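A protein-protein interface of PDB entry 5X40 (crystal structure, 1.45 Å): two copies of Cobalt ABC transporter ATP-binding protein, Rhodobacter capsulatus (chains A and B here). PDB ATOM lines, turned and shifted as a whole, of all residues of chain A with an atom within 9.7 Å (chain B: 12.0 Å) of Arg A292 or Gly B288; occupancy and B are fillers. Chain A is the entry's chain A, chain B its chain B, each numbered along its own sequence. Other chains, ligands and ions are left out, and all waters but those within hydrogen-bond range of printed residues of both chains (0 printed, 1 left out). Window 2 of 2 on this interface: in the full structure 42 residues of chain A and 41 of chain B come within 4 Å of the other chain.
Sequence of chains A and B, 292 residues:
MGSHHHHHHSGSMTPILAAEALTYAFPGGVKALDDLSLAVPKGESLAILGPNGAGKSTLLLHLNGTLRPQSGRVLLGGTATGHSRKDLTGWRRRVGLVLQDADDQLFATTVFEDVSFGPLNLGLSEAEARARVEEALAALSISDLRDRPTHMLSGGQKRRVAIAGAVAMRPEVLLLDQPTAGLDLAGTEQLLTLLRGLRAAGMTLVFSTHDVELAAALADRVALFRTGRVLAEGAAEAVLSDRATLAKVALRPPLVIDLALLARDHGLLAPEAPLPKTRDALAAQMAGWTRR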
ATOM      1  N   ALA A 263      -8.722 -18.989  14.566  1.00  0.00           N
ATOM      2  CA  ALA A 263      -8.272 -17.605  14.647  1.00  0.00           C
ATOM      3  C   ALA A 263      -7.371 -17.397  15.863  1.00  0.00           C
ATOM      4  O   ALA A 263      -6.347 -16.722  15.776  1.00  0.00           O
ATOM      5  CB  ALA A 263      -9.470 -16.661  14.695  1.00  0.00           C
ATOM      6  N   ARG A 264      -7.745 -17.998  16.990  1.00  0.00           N
ATOM      7  CA  ARG A 264      -6.952 -17.897  18.214  1.00  0.00           C
ATOM      8  C   ARG A 264      -5.605 -18.597  18.045  1.00  0.00           C
ATOM      9  O   ARG A 264      -4.588 -18.139  18.574  1.00  0.00           O
ATOM     10  CB  ARG A 264      -7.721 -18.485  19.404  1.00  0.00           C
ATOM     11  CG  ARG A 264      -6.976 -18.422  20.731  1.00  0.00           C
ATOM     12  CD  ARG A 264      -7.935 -18.469  21.912  1.00  0.00           C
ATOM     13  NE  ARG A 264      -8.256 -19.831  22.331  1.00  0.00           N
ATOM     14  CZ  ARG A 264      -9.206 -20.134  23.211  1.00  0.00           C
ATOM     15  NH1 ARG A 264      -9.434 -21.401  23.542  1.00  0.00           N
ATOM     16  NH2 ARG A 264      -9.934 -19.170  23.761  1.00  0.00           N
ATOM     17  N   ASP A 265      -5.605 -19.695  17.289  1.00  0.00           N
ATOM     18  CA  ASP A 265      -4.387 -20.454  17.006  1.00  0.00           C
ATOM     19  C   ASP A 265      -3.368 -19.561  16.301  1.00  0.00           C
ATOM     20  O   ASP A 265      -2.159 -19.737  16.451  1.00  0.00           O
ATOM     21  CB  ASP A 265      -4.716 -21.698  16.160  1.00  0.00           C
ATOM     22  CG  ASP A 265      -3.473 -22.436  15.664  1.00  0.00           C
ATOM     23  OD1 ASP A 265      -2.879 -23.218  16.440  1.00  0.00           O
ATOM     24  OD2 ASP A 265      -3.104 -22.251  14.482  1.00  0.00           O
ATOM     25  N   HIS A 266      -3.868 -18.579  15.558  1.00  0.00           N
ATOM     26  CA  HIS A 266      -3.010 -17.644  14.843  1.00  0.00           C
ATOM     27  C   HIS A 266      -2.942 -16.273  15.518  1.00  0.00           C
ATOM     28  O   HIS A 266      -2.476 -15.304  14.919  1.00  0.00           O
ATOM     29  CB  HIS A 266      -3.487 -17.504  13.399  1.00  0.00           C
ATOM     30  CG  HIS A 266      -3.329 -18.757  12.596  1.00  0.00           C
ATOM     31  ND1 HIS A 266      -4.305 -19.728  12.532  1.00  0.00           N
ATOM     32  CD2 HIS A 266      -2.300 -19.208  11.841  1.00  0.00           C
ATOM     33  CE1 HIS A 266      -3.888 -20.718  11.763  1.00  0.00           C
ATOM     34  NE2 HIS A 266      -2.674 -20.428  11.332  1.00  0.00           N
ATOM     35  N   GLY A 267      -3.400 -16.203  16.764  1.00  0.00           N
ATOM     36  CA  GLY A 267      -3.305 -14.988  17.557  1.00  0.00           C
ATOM     37  C   GLY A 267      -4.141 -13.819  17.063  1.00  0.00           C
ATOM     38  O   GLY A 267      -3.856 -12.666  17.380  1.00  0.00           O
ATOM     39  N   LEU A 268      -5.188 -14.112  16.301  1.00  0.00           N
ATOM     40  CA  LEU A 268      -6.025 -13.069  15.719  1.00  0.00           C
ATOM     41  C   LEU A 268      -7.138 -12.618  16.665  1.00  0.00           C
ATOM     42  O   LEU A 268      -7.856 -11.660  16.372  1.00  0.00           O
ATOM     43  CB  LEU A 268      -6.623 -13.549  14.394  1.00  0.00           C
ATOM     44  CG  LEU A 268      -5.636 -13.820  13.256  1.00  0.00           C
ATOM     45  CD1 LEU A 268      -6.337 -14.449  12.062  1.00  0.00           C
ATOM     46  CD2 LEU A 268      -4.931 -12.536  12.848  1.00  0.00           C
ATOM     47  N   TRP A 289      -8.412  -7.021  11.659  1.00  0.00           N
ATOM     48  CA  TRP A 289      -7.287  -7.766  11.104  1.00  0.00           C
ATOM     49  C   TRP A 289      -6.623  -7.044   9.940  1.00  0.00           C
ATOM     50  O   TRP A 289      -7.287  -6.381   9.146  1.00  0.00           O
ATOM     51  CB  TRP A 289      -7.735  -9.152  10.651  1.00  0.00           C
ATOM     52  CG  TRP A 289      -8.209 -10.009  11.768  1.00  0.00           C
ATOM     53  CD1 TRP A 289      -8.051  -9.779  13.106  1.00  0.00           C
ATOM     54  CD2 TRP A 289      -8.936 -11.234  11.653  1.00  0.00           C
ATOM     55  NE1 TRP A 289      -8.632 -10.794  13.829  1.00  0.00           N
ATOM     56  CE2 TRP A 289      -9.183 -11.699  12.960  1.00  0.00           C
ATOM     57  CE3 TRP A 289      -9.397 -11.988  10.569  1.00  0.00           C
ATOM     58  CZ2 TRP A 289      -9.875 -12.883  13.214  1.00  0.00           C
ATOM     59  CZ3 TRP A 289     -10.085 -13.164  10.823  1.00  0.00           C
ATOM     60  CH2 TRP A 289     -10.316 -13.599  12.135  1.00  0.00           C
ATOM     61  N   THR A 290      -5.307  -7.192   9.842  1.00  0.00           N
ATOM     62  CA  THR A 290      -4.561  -6.654   8.714  1.00  0.00           C
ATOM     63  C   THR A 290      -3.551  -7.666   8.187  1.00  0.00           C
ATOM     64  O   THR A 290      -3.175  -8.604   8.887  1.00  0.00           O
ATOM     65  CB  THR A 290      -3.819  -5.362   9.086  1.00  0.00           C
ATOM     66  OG1 THR A 290      -3.156  -4.846   7.927  1.00  0.00           O
ATOM     67  CG2 THR A 290      -2.784  -5.625  10.180  1.00  0.00           C
ATOM     68  N   ARG A 291      -3.113  -7.471   6.948  1.00  0.00           N
ATOM     69  CA  ARG A 291      -2.078  -8.321   6.372  1.00  0.00           C
ATOM     70  C   ARG A 291      -0.713  -7.987   6.961  1.00  0.00           C
ATOM     71  O   ARG A 291      -0.469  -6.857   7.384  1.00  0.00           O
ATOM     72  CB  ARG A 291      -2.037  -8.163   4.853  1.00  0.00           C
ATOM     73  CG  ARG A 291      -3.276  -8.682   4.152  1.00  0.00           C
ATOM     74  CD  ARG A 291      -3.212  -8.425   2.658  1.00  0.00           C
ATOM     75  NE  ARG A 291      -2.082  -9.112   2.043  1.00  0.00           N
ATOM     76  CZ  ARG A 291      -2.098 -10.384   1.659  1.00  0.00           C
ATOM     77  NH1 ARG A 291      -1.019 -10.923   1.109  1.00  0.00           N
ATOM     78  NH2 ARG A 291      -3.190 -11.119   1.827  1.00  0.00           N
ATOM     79  N   ARG A 292       0.170  -8.976   6.984  1.00  0.00           N
ATOM     80  CA  ARG A 292       1.540  -8.761   7.426  1.00  0.00           C
ATOM     81  C   ARG A 292       2.368  -8.123   6.315  1.00  0.00           C
ATOM     82  O   ARG A 292       1.846  -7.809   5.243  1.00  0.00           O
ATOM     83  CB  ARG A 292       2.169 -10.082   7.867  1.00  0.00           C
ATOM     84  CG  ARG A 292       1.481 -10.731   9.063  1.00  0.00           C
ATOM     85  CD  ARG A 292       1.927 -12.175   9.209  1.00  0.00           C
ATOM     86  NE  ARG A 292       1.946 -12.614  10.601  1.00  0.00           N
ATOM     87  CZ  ARG A 292       1.033 -13.406  11.152  1.00  0.00           C
ATOM     88  NH1 ARG A 292       0.014 -13.847  10.431  1.00  0.00           N
ATOM     89  NH2 ARG A 292       1.136 -13.751  12.428  1.00  0.00           N
ATOM     90  N   ALA B 263     -13.236 -10.694   3.995  1.00  0.00           N
ATOM     91  CA  ALA B 263     -11.787 -10.552   3.901  1.00  0.00           C
ATOM     92  C   ALA B 263     -11.389  -9.831   2.619  1.00  0.00           C
ATOM     93  O   ALA B 263     -10.511  -8.969   2.620  1.00  0.00           O
ATOM     94  CB  ALA B 263     -11.117 -11.918   3.968  1.00  0.00           C
ATOM     95  N   HIS B 266     -12.205  -6.234   2.993  1.00  0.00           N
ATOM     96  CA  HIS B 266     -11.337  -5.638   3.998  1.00  0.00           C
ATOM     97  C   HIS B 266      -9.903  -5.483   3.499  1.00  0.00           C
ATOM     98  O   HIS B 266      -9.078  -4.853   4.158  1.00  0.00           O
ATOM     99  CB  HIS B 266     -11.340  -6.486   5.273  1.00  0.00           C
ATOM    100  CG  HIS B 266     -12.502  -6.234   6.185  1.00  0.00           C
ATOM    101  ND1 HIS B 266     -12.694  -5.034   6.834  1.00  0.00           N
ATOM    102  CD2 HIS B 266     -13.512  -7.043   6.588  1.00  0.00           C
ATOM    103  CE1 HIS B 266     -13.780  -5.108   7.582  1.00  0.00           C
ATOM    104  NE2 HIS B 266     -14.296  -6.316   7.450  1.00  0.00           N
ATOM    105  N   GLY B 267      -9.605  -6.071   2.344  1.00  0.00           N
ATOM    106  CA  GLY B 267      -8.270  -6.015   1.775  1.00  0.00           C
ATOM    107  C   GLY B 267      -7.308  -7.054   2.328  1.00  0.00           C
ATOM    108  O   GLY B 267      -6.094  -6.929   2.164  1.00  0.00           O
ATOM    109  N   LEU B 268      -7.831  -8.109   2.921  1.00  0.00           N
ATOM    110  CA  LEU B 268      -7.023  -9.155   3.488  1.00  0.00           C
ATOM    111  C   LEU B 268      -6.515 -10.134   2.467  1.00  0.00           C
ATOM    112  O   LEU B 268      -5.692 -10.963   2.770  1.00  0.00           O
ATOM    113  CB  LEU B 268      -7.811  -9.905   4.532  1.00  0.00           C
ATOM    114  CG  LEU B 268      -7.879  -9.421   5.961  1.00  0.00           C
ATOM    115  CD1 LEU B 268      -6.493  -9.200   6.522  1.00  0.00           C
ATOM    116  CD2 LEU B 268      -8.678  -8.165   6.002  1.00  0.00           C
ATOM    117  N   LEU B 269      -7.033 -10.061   1.266  1.00  0.00           N
ATOM    118  CA  LEU B 269      -6.631 -11.015   0.267  1.00  0.00           C
ATOM    119  C   LEU B 269      -5.736 -10.373  -0.749  1.00  0.00           C
ATOM    120  O   LEU B 269      -6.065  -9.369  -1.301  1.00  0.00           O
ATOM    121  CB  LEU B 269      -7.825 -11.627  -0.437  1.00  0.00           C
ATOM    122  CG  LEU B 269      -8.830 -12.344   0.420  1.00  0.00           C
ATOM    123  CD1 LEU B 269      -9.886 -12.870  -0.502  1.00  0.00           C
ATOM    124  CD2 LEU B 269      -8.148 -13.486   1.136  1.00  0.00           C
ATOM    125  N   ALA B 270      -4.599 -10.951  -1.034  1.00  0.00           N
ATOM    126  CA  ALA B 270      -3.810 -10.368  -2.105  1.00  0.00           C
ATOM    127  C   ALA B 270      -3.647  -8.824  -2.001  1.00  0.00           C
ATOM    128  O   ALA B 270      -2.923  -8.289  -1.154  1.00  0.00           O
ATOM    129  CB  ALA B 270      -4.468 -10.701  -3.433  1.00  0.00           C
ATOM    130  N   PRO B 271      -4.255  -8.133  -2.971  1.00  0.00           N
ATOM    131  CA  PRO B 271      -5.220  -8.717  -3.919  1.00  0.00           C
ATOM    132  C   PRO B 271      -4.782  -9.419  -5.208  1.00  0.00           C
ATOM    133  O   PRO B 271      -3.656  -9.340  -5.647  1.00  0.00           O
ATOM    134  CB  PRO B 271      -6.102  -7.507  -4.299  1.00  0.00           C
ATOM    135  CG  PRO B 271      -5.483  -6.329  -3.666  1.00  0.00           C
ATOM    136  CD  PRO B 271      -4.735  -6.838  -2.481  1.00  0.00           C
ATOM    137  N   ALA B 273      -6.136 -12.744  -5.535  1.00  0.00           N
ATOM    138  CA  ALA B 273      -6.175 -14.157  -5.097  1.00  0.00           C
ATOM    139  C   ALA B 273      -7.559 -14.763  -5.119  1.00  0.00           C
ATOM    140  O   ALA B 273      -8.525 -14.025  -5.052  1.00  0.00           O
ATOM    141  CB  ALA B 273      -5.605 -14.271  -3.694  1.00  0.00           C
ATOM    142  N   PRO B 276     -11.069 -18.120  -0.584  1.00  0.00           N
ATOM    143  CA  PRO B 276     -11.119 -19.339   0.247  1.00  0.00           C
ATOM    144  C   PRO B 276     -12.558 -19.801   0.501  1.00  0.00           C
ATOM    145  O   PRO B 276     -13.404 -19.025   0.959  1.00  0.00           O
ATOM    146  CB  PRO B 276     -10.427 -18.921   1.560  1.00  0.00           C
ATOM    147  CG  PRO B 276     -10.379 -17.436   1.544  1.00  0.00           C
ATOM    148  CD  PRO B 276     -10.372 -17.014   0.096  1.00  0.00           C
ATOM    149  N   ARG B 279     -12.557 -24.478   5.130  1.00  0.00           N
ATOM    150  CA  ARG B 279     -11.846 -24.292   6.379  1.00  0.00           C
ATOM    151  C   ARG B 279     -10.331 -24.328   6.164  1.00  0.00           C
ATOM    152  O   ARG B 279      -9.596 -23.480   6.681  1.00  0.00           O
ATOM    153  CB  ARG B 279     -12.269 -25.375   7.366  1.00  0.00           C
ATOM    154  CG  ARG B 279     -11.883 -25.099   8.781  1.00  0.00           C
ATOM    155  CD  ARG B 279     -10.598 -25.802   9.185  1.00  0.00           C
ATOM    156  NE  ARG B 279     -10.446 -25.662  10.622  1.00  0.00           N
ATOM    157  CZ  ARG B 279      -9.289 -25.649  11.275  1.00  0.00           C
ATOM    158  NH1 ARG B 279      -9.296 -25.519  12.591  1.00  0.00           N
ATOM    159  NH2 ARG B 279      -8.135 -25.765  10.624  1.00  0.00           N
ATOM    160  N   ASP B 280      -9.877 -25.306   5.386  1.00  0.00           N
ATOM    161  CA  ASP B 280      -8.454 -25.455   5.085  1.00  0.00           C
ATOM    162  C   ASP B 280      -7.905 -24.222   4.390  1.00  0.00           C
ATOM    163  O   ASP B 280      -6.809 -23.764   4.695  1.00  0.00           O
ATOM    164  CB  ASP B 280      -8.199 -26.677   4.201  1.00  0.00           C
ATOM    165  CG  ASP B 280      -8.498 -27.983   4.894  1.00  0.00           C
ATOM    166  OD1 ASP B 280      -8.469 -28.049   6.143  1.00  0.00           O
ATOM    167  OD2 ASP B 280      -8.746 -28.954   4.162  1.00  0.00           O
ATOM    168  N   ALA B 281      -8.677 -23.685   3.450  1.00  0.00           N
ATOM    169  CA  ALA B 281      -8.213 -22.559   2.658  1.00  0.00           C
ATOM    170  C   ALA B 281      -8.154 -21.310   3.520  1.00  0.00           C
ATOM    171  O   ALA B 281      -7.219 -20.517   3.427  1.00  0.00           O
ATOM    172  CB  ALA B 281      -9.118 -22.337   1.450  1.00  0.00           C
ATOM    173  N   LEU B 282      -9.156 -21.149   4.377  1.00  0.00           N
ATOM    174  CA  LEU B 282      -9.218 -19.977   5.233  1.00  0.00           C
ATOM    175  C   LEU B 282      -8.107 -20.039   6.272  1.00  0.00           C
ATOM    176  O   LEU B 282      -7.470 -19.028   6.567  1.00  0.00           O
ATOM    177  CB  LEU B 282     -10.594 -19.870   5.894  1.00  0.00           C
ATOM    178  CG  LEU B 282     -10.864 -18.620   6.728  1.00  0.00           C
ATOM    179  CD1 LEU B 282     -10.789 -17.357   5.867  1.00  0.00           C
ATOM    180  CD2 LEU B 282     -12.221 -18.734   7.372  1.00  0.00           C
ATOM    181  N   ALA B 283      -7.855 -21.235   6.802  1.00  0.00           N
ATOM    182  CA  ALA B 283      -6.787 -21.436   7.780  1.00  0.00           C
ATOM    183  C   ALA B 283      -5.440 -21.027   7.210  1.00  0.00           C
ATOM    184  O   ALA B 283      -4.623 -20.392   7.891  1.00  0.00           O
ATOM    185  CB  ALA B 283      -6.738 -22.895   8.235  1.00  0.00           C
ATOM    186  N   ALA B 284      -5.205 -21.407   5.960  1.00  0.00           N
ATOM    187  CA  ALA B 284      -3.953 -21.074   5.299  1.00  0.00           C
ATOM    188  C   ALA B 284      -3.796 -19.562   5.157  1.00  0.00           C
ATOM    189  O   ALA B 284      -2.689 -19.041   5.260  1.00  0.00           O
ATOM    190  CB  ALA B 284      -3.870 -21.755   3.939  1.00  0.00           C
ATOM    191  N   GLN B 285      -4.899 -18.855   4.936  1.00  0.00           N
ATOM    192  CA  GLN B 285      -4.829 -17.404   4.788  1.00  0.00           C
ATOM    193  C   GLN B 285      -4.510 -16.708   6.105  1.00  0.00           C
ATOM    194  O   GLN B 285      -3.786 -15.708   6.132  1.00  0.00           O
ATOM    195  CB  GLN B 285      -6.139 -16.855   4.222  1.00  0.00           C
ATOM    196  CG  GLN B 285      -6.395 -17.253   2.785  1.00  0.00           C
ATOM    197  CD  GLN B 285      -5.313 -16.749   1.854  1.00  0.00           C
ATOM    198  OE1 GLN B 285      -4.731 -17.517   1.089  1.00  0.00           O
ATOM    199  NE2 GLN B 285      -5.036 -15.452   1.914  1.00  0.00           N
ATOM    200  N   MET B 286      -5.055 -17.241   7.192  1.00  0.00           N
ATOM    201  CA  MET B 286      -4.915 -16.638   8.513  1.00  0.00           C
ATOM    202  C   MET B 286      -3.473 -16.443   8.951  1.00  0.00           C
ATOM    203  O   MET B 286      -3.170 -15.512   9.693  1.00  0.00           O
ATOM    204  CB  MET B 286      -5.641 -17.486   9.546  1.00  0.00           C
ATOM    205  CG  MET B 286      -7.137 -17.449   9.397  1.00  0.00           C
ATOM    206  SD  MET B 286      -7.935 -18.066  10.880  1.00  0.00           S
ATOM    207  CE  MET B 286      -9.630 -17.605  10.576  1.00  0.00           C
ATOM    208  N   ALA B 287      -2.586 -17.321   8.496  1.00  0.00           N
ATOM    209  CA  ALA B 287      -1.179 -17.244   8.870  1.00  0.00           C
ATOM    210  C   ALA B 287      -0.508 -15.976   8.326  1.00  0.00           C
ATOM    211  O   ALA B 287       0.546 -15.569   8.811  1.00  0.00           O
ATOM    212  CB  ALA B 287      -0.440 -18.484   8.390  1.00  0.00           C
ATOM    213  N   GLY B 288      -1.127 -15.349   7.329  1.00  0.00           N
ATOM    214  CA  GLY B 288      -0.608 -14.119   6.754  1.00  0.00           C
ATOM    215  C   GLY B 288      -1.288 -12.875   7.300  1.00  0.00           C
ATOM    216  O   GLY B 288      -1.129 -11.773   6.767  1.00  0.00           O
ATOM    217  N   TRP B 289      -2.049 -13.056   8.375  1.00  0.00           N
ATOM    218  CA  TRP B 289      -2.780 -11.964   8.999  1.00  0.00           C
ATOM    219  C   TRP B 289      -2.299 -11.696  10.419  1.00  0.00           C
ATOM    220  O   TRP B 289      -1.840 -12.604  11.109  1.00  0.00           O
ATOM    221  CB  TRP B 289      -4.276 -12.278   9.032  1.00  0.00           C
ATOM    222  CG  TRP B 289      -4.905 -12.435   7.691  1.00  0.00           C
ATOM    223  CD1 TRP B 289      -4.396 -12.041   6.486  1.00  0.00           C
ATOM    224  CD2 TRP B 289      -6.169 -13.040   7.415  1.00  0.00           C
ATOM    225  NE1 TRP B 289      -5.271 -12.360   5.475  1.00  0.00           N
ATOM    226  CE2 TRP B 289      -6.367 -12.976   6.021  1.00  0.00           C
ATOM    227  CE3 TRP B 289      -7.156 -13.629   8.213  1.00  0.00           C
ATOM    228  CZ2 TRP B 289      -7.513 -13.478   5.408  1.00  0.00           C
ATOM    229  CZ3 TRP B 289      -8.291 -14.125   7.604  1.00  0.00           C
ATOM    230  CH2 TRP B 289      -8.461 -14.050   6.215  1.00  0.00           C
ATOM    231  N   THR B 290      -2.414 -10.446  10.851  1.00  0.00           N
ATOM    232  CA  THR B 290      -2.233 -10.102  12.257  1.00  0.00           C
ATOM    233  C   THR B 290      -3.297  -9.112  12.699  1.00  0.00           C
ATOM    234  O   THR B 290      -4.081  -8.608  11.894  1.00  0.00           O
ATOM    235  CB  THR B 290      -0.838  -9.492  12.563  1.00  0.00           C
ATOM    236  OG1 THR B 290      -0.391  -8.696  11.457  1.00  0.00           O
ATOM    237  CG2 THR B 290       0.182 -10.578  12.847  1.00  0.00           C
ATOM    238  N   ARG B 291      -3.310  -8.839  13.994  1.00  0.00           N
ATOM    239  CA  ARG B 291      -4.225  -7.877  14.573  1.00  0.00           C
ATOM    240  C   ARG B 291      -3.672  -6.460  14.428  1.00  0.00           C
ATOM    241  O   ARG B 291      -2.460  -6.253  14.491  1.00  0.00           O
ATOM    242  CB  ARG B 291      -4.468  -8.220  16.040  1.00  0.00           C
ATOM    243  CG  ARG B 291      -5.256  -7.190  16.806  1.00  0.00           C
ATOM    244  CD  ARG B 291      -5.910  -7.815  18.014  1.00  0.00           C
ATOM    245  NE  ARG B 291      -7.215  -8.382  17.696  1.00  0.00           N
ATOM    246  CZ  ARG B 291      -8.186  -8.534  18.590  1.00  0.00           C
ATOM    247  NH1 ARG B 291      -9.355  -9.055  18.237  1.00  0.00           N
ATOM    248  NH2 ARG B 291      -7.983  -8.150  19.840  1.00  0.00           N
ATOM    249  N   ARG B 292      -4.566  -5.496  14.219  1.00  0.00           N
ATOM    250  CA  ARG B 292      -4.186  -4.090  14.126  1.00  0.00           C
ATOM    251  C   ARG B 292      -3.744  -3.549  15.485  1.00  0.00           C
ATOM    252  O   ARG B 292      -4.157  -4.055  16.531  1.00  0.00           O
ATOM    253  CB  ARG B 292      -5.350  -3.259  13.581  1.00  0.00           C
ATOM    254  CG  ARG B 292      -5.192  -2.828  12.131  1.00  0.00           C
ATOM    255  CD  ARG B 292      -6.493  -2.262  11.586  1.00  0.00           C
ATOM    256  NE  ARG B 292      -6.944  -1.096  12.342  1.00  0.00           N
ATOM    257  CZ  ARG B 292      -8.219  -0.748  12.492  1.00  0.00           C
ATOM    258  NH1 ARG B 292      -9.179  -1.480  11.942  1.00  0.00           N
ATOM    259  NH2 ARG B 292      -8.537   0.330  13.199  1.00  0.00           N
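Of chain B, only Met B286, Ala B287, Gly B288, Trp B289 and Thr B290 come within 4 Å of Arg A292. Gly B288 touches two residues of chain A. Of chain B, only Ala B283 (3.95 Å), Met B286 (3.97 Å) and Ala B287 (3.7 Å) come within 4 Å of His A266. Of chain B, only Leu B268 (3.7 Å), Trp B289 (3.4 Å) and Thr B290 (2.8 Å) come within 4 Å of Thr A290. Arg A291 touches five residues of chain B. Printed residues of chain A within 4 Å of Ala B287: His A266 and Arg A292. Printed residues of chain A within 4 Å of Trp B289: Leu A268, Trp A289, Thr A290 and Arg A292. Of the printed residues of chain A, Met B286 touches Ala A263, His A266 and Arg A292. Pro B271 touches none of the printed residues of chain A. Asp B280 touches none of the printed residues of chain A. The nearest residue of chain B that does not touch Arg A292 is Gln B285 (6.0 Å).
The backbone NH of Thr A290 is in hydrogen-bond range of the backbone carbonyl oxygen of Thr B290 (2.8 Å). The guanidinium group of Arg A291 sits at hydrogen-bond distance from the backbone carbonyl oxygen of Leu B268 (2.7 Å). The guanidinium group (NE) of Arg A291 lies within hydrogen-bond range of the backbone carbonyl oxygen (O) of Ala B270 (3.4 Å). The backbone carbonyl oxygen (O) of Ala B287 lies within hydrogen-bond range of the guanidinium group (NH1) of Arg A292 (2.4 Å). The backbone NH of Arg A292 lies within hydrogen-bond range of the backbone carbonyl oxygen of Gly B288 (3.1 Å). O of Trp B289 lies close to NH2 of Arg A292.
Leu A268 touches Thr B290, and with the chains exchanged Thr A290 touches Leu B268. Trp A289 touches Thr B290, and with the chains exchanged Thr A290 touches Trp B289. Thr B290 touches its own counterpart, Thr A290. Arg A291 touches Gly B267, but with the chains exchanged Gly A267 does not touch Arg B291 (4.7 Å).
N of Leu A268 sits at hydrogen-bond distance from O of Ala A263, 2.9 Å away. A ring nitrogen (ND1) of His A266 lies close to the side-chain carboxylate of Asp A265, at 3.4 Å. O of Leu A268 sits at hydrogen-bond distance from NE1 of Trp A289 (2.8 Å). O of Ala B263 lies within hydrogen-bond range of N of Leu B268. O of Leu B268 lies within hydrogen-bond range of NE1 of Trp B289, 3.1 Å away.
Among the printed residues, pairs that only touch across the chains: Arg A291 with Gly B267, Arg A292 with Thr B290, Thr A290 with Trp B289, Trp A289 with Thr B290, Leu A268 with Arg B291, Leu A268 with Trp B289, Arg A291 with Gly B288, Trp A289 with Trp B289, Arg A292 with Met B286, Leu A268 with Thr B290, Arg A291 with Leu B269, Thr A290 with Leu B268, His A266 with Ala B287, Ala A263 with Met B286, Trp A289 with Leu B268, His A266 with Ala B283 and His A266 with Met B286.
Printed residues of chain B that touch a printed residue of chain A: Gly B267, Leu B268, Leu B269, Ala B270, Ala B283, Met B286, Ala B287, Gly B288, Trp B289, Thr B290 and Arg B291. Of the 10 printed residues of chain A, 7 touch a printed residue of chain B. Among the printed residues, no Asp or Glu carboxylate lies within 4 Å of a Lys or Arg side-chain nitrogen of the other chain.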
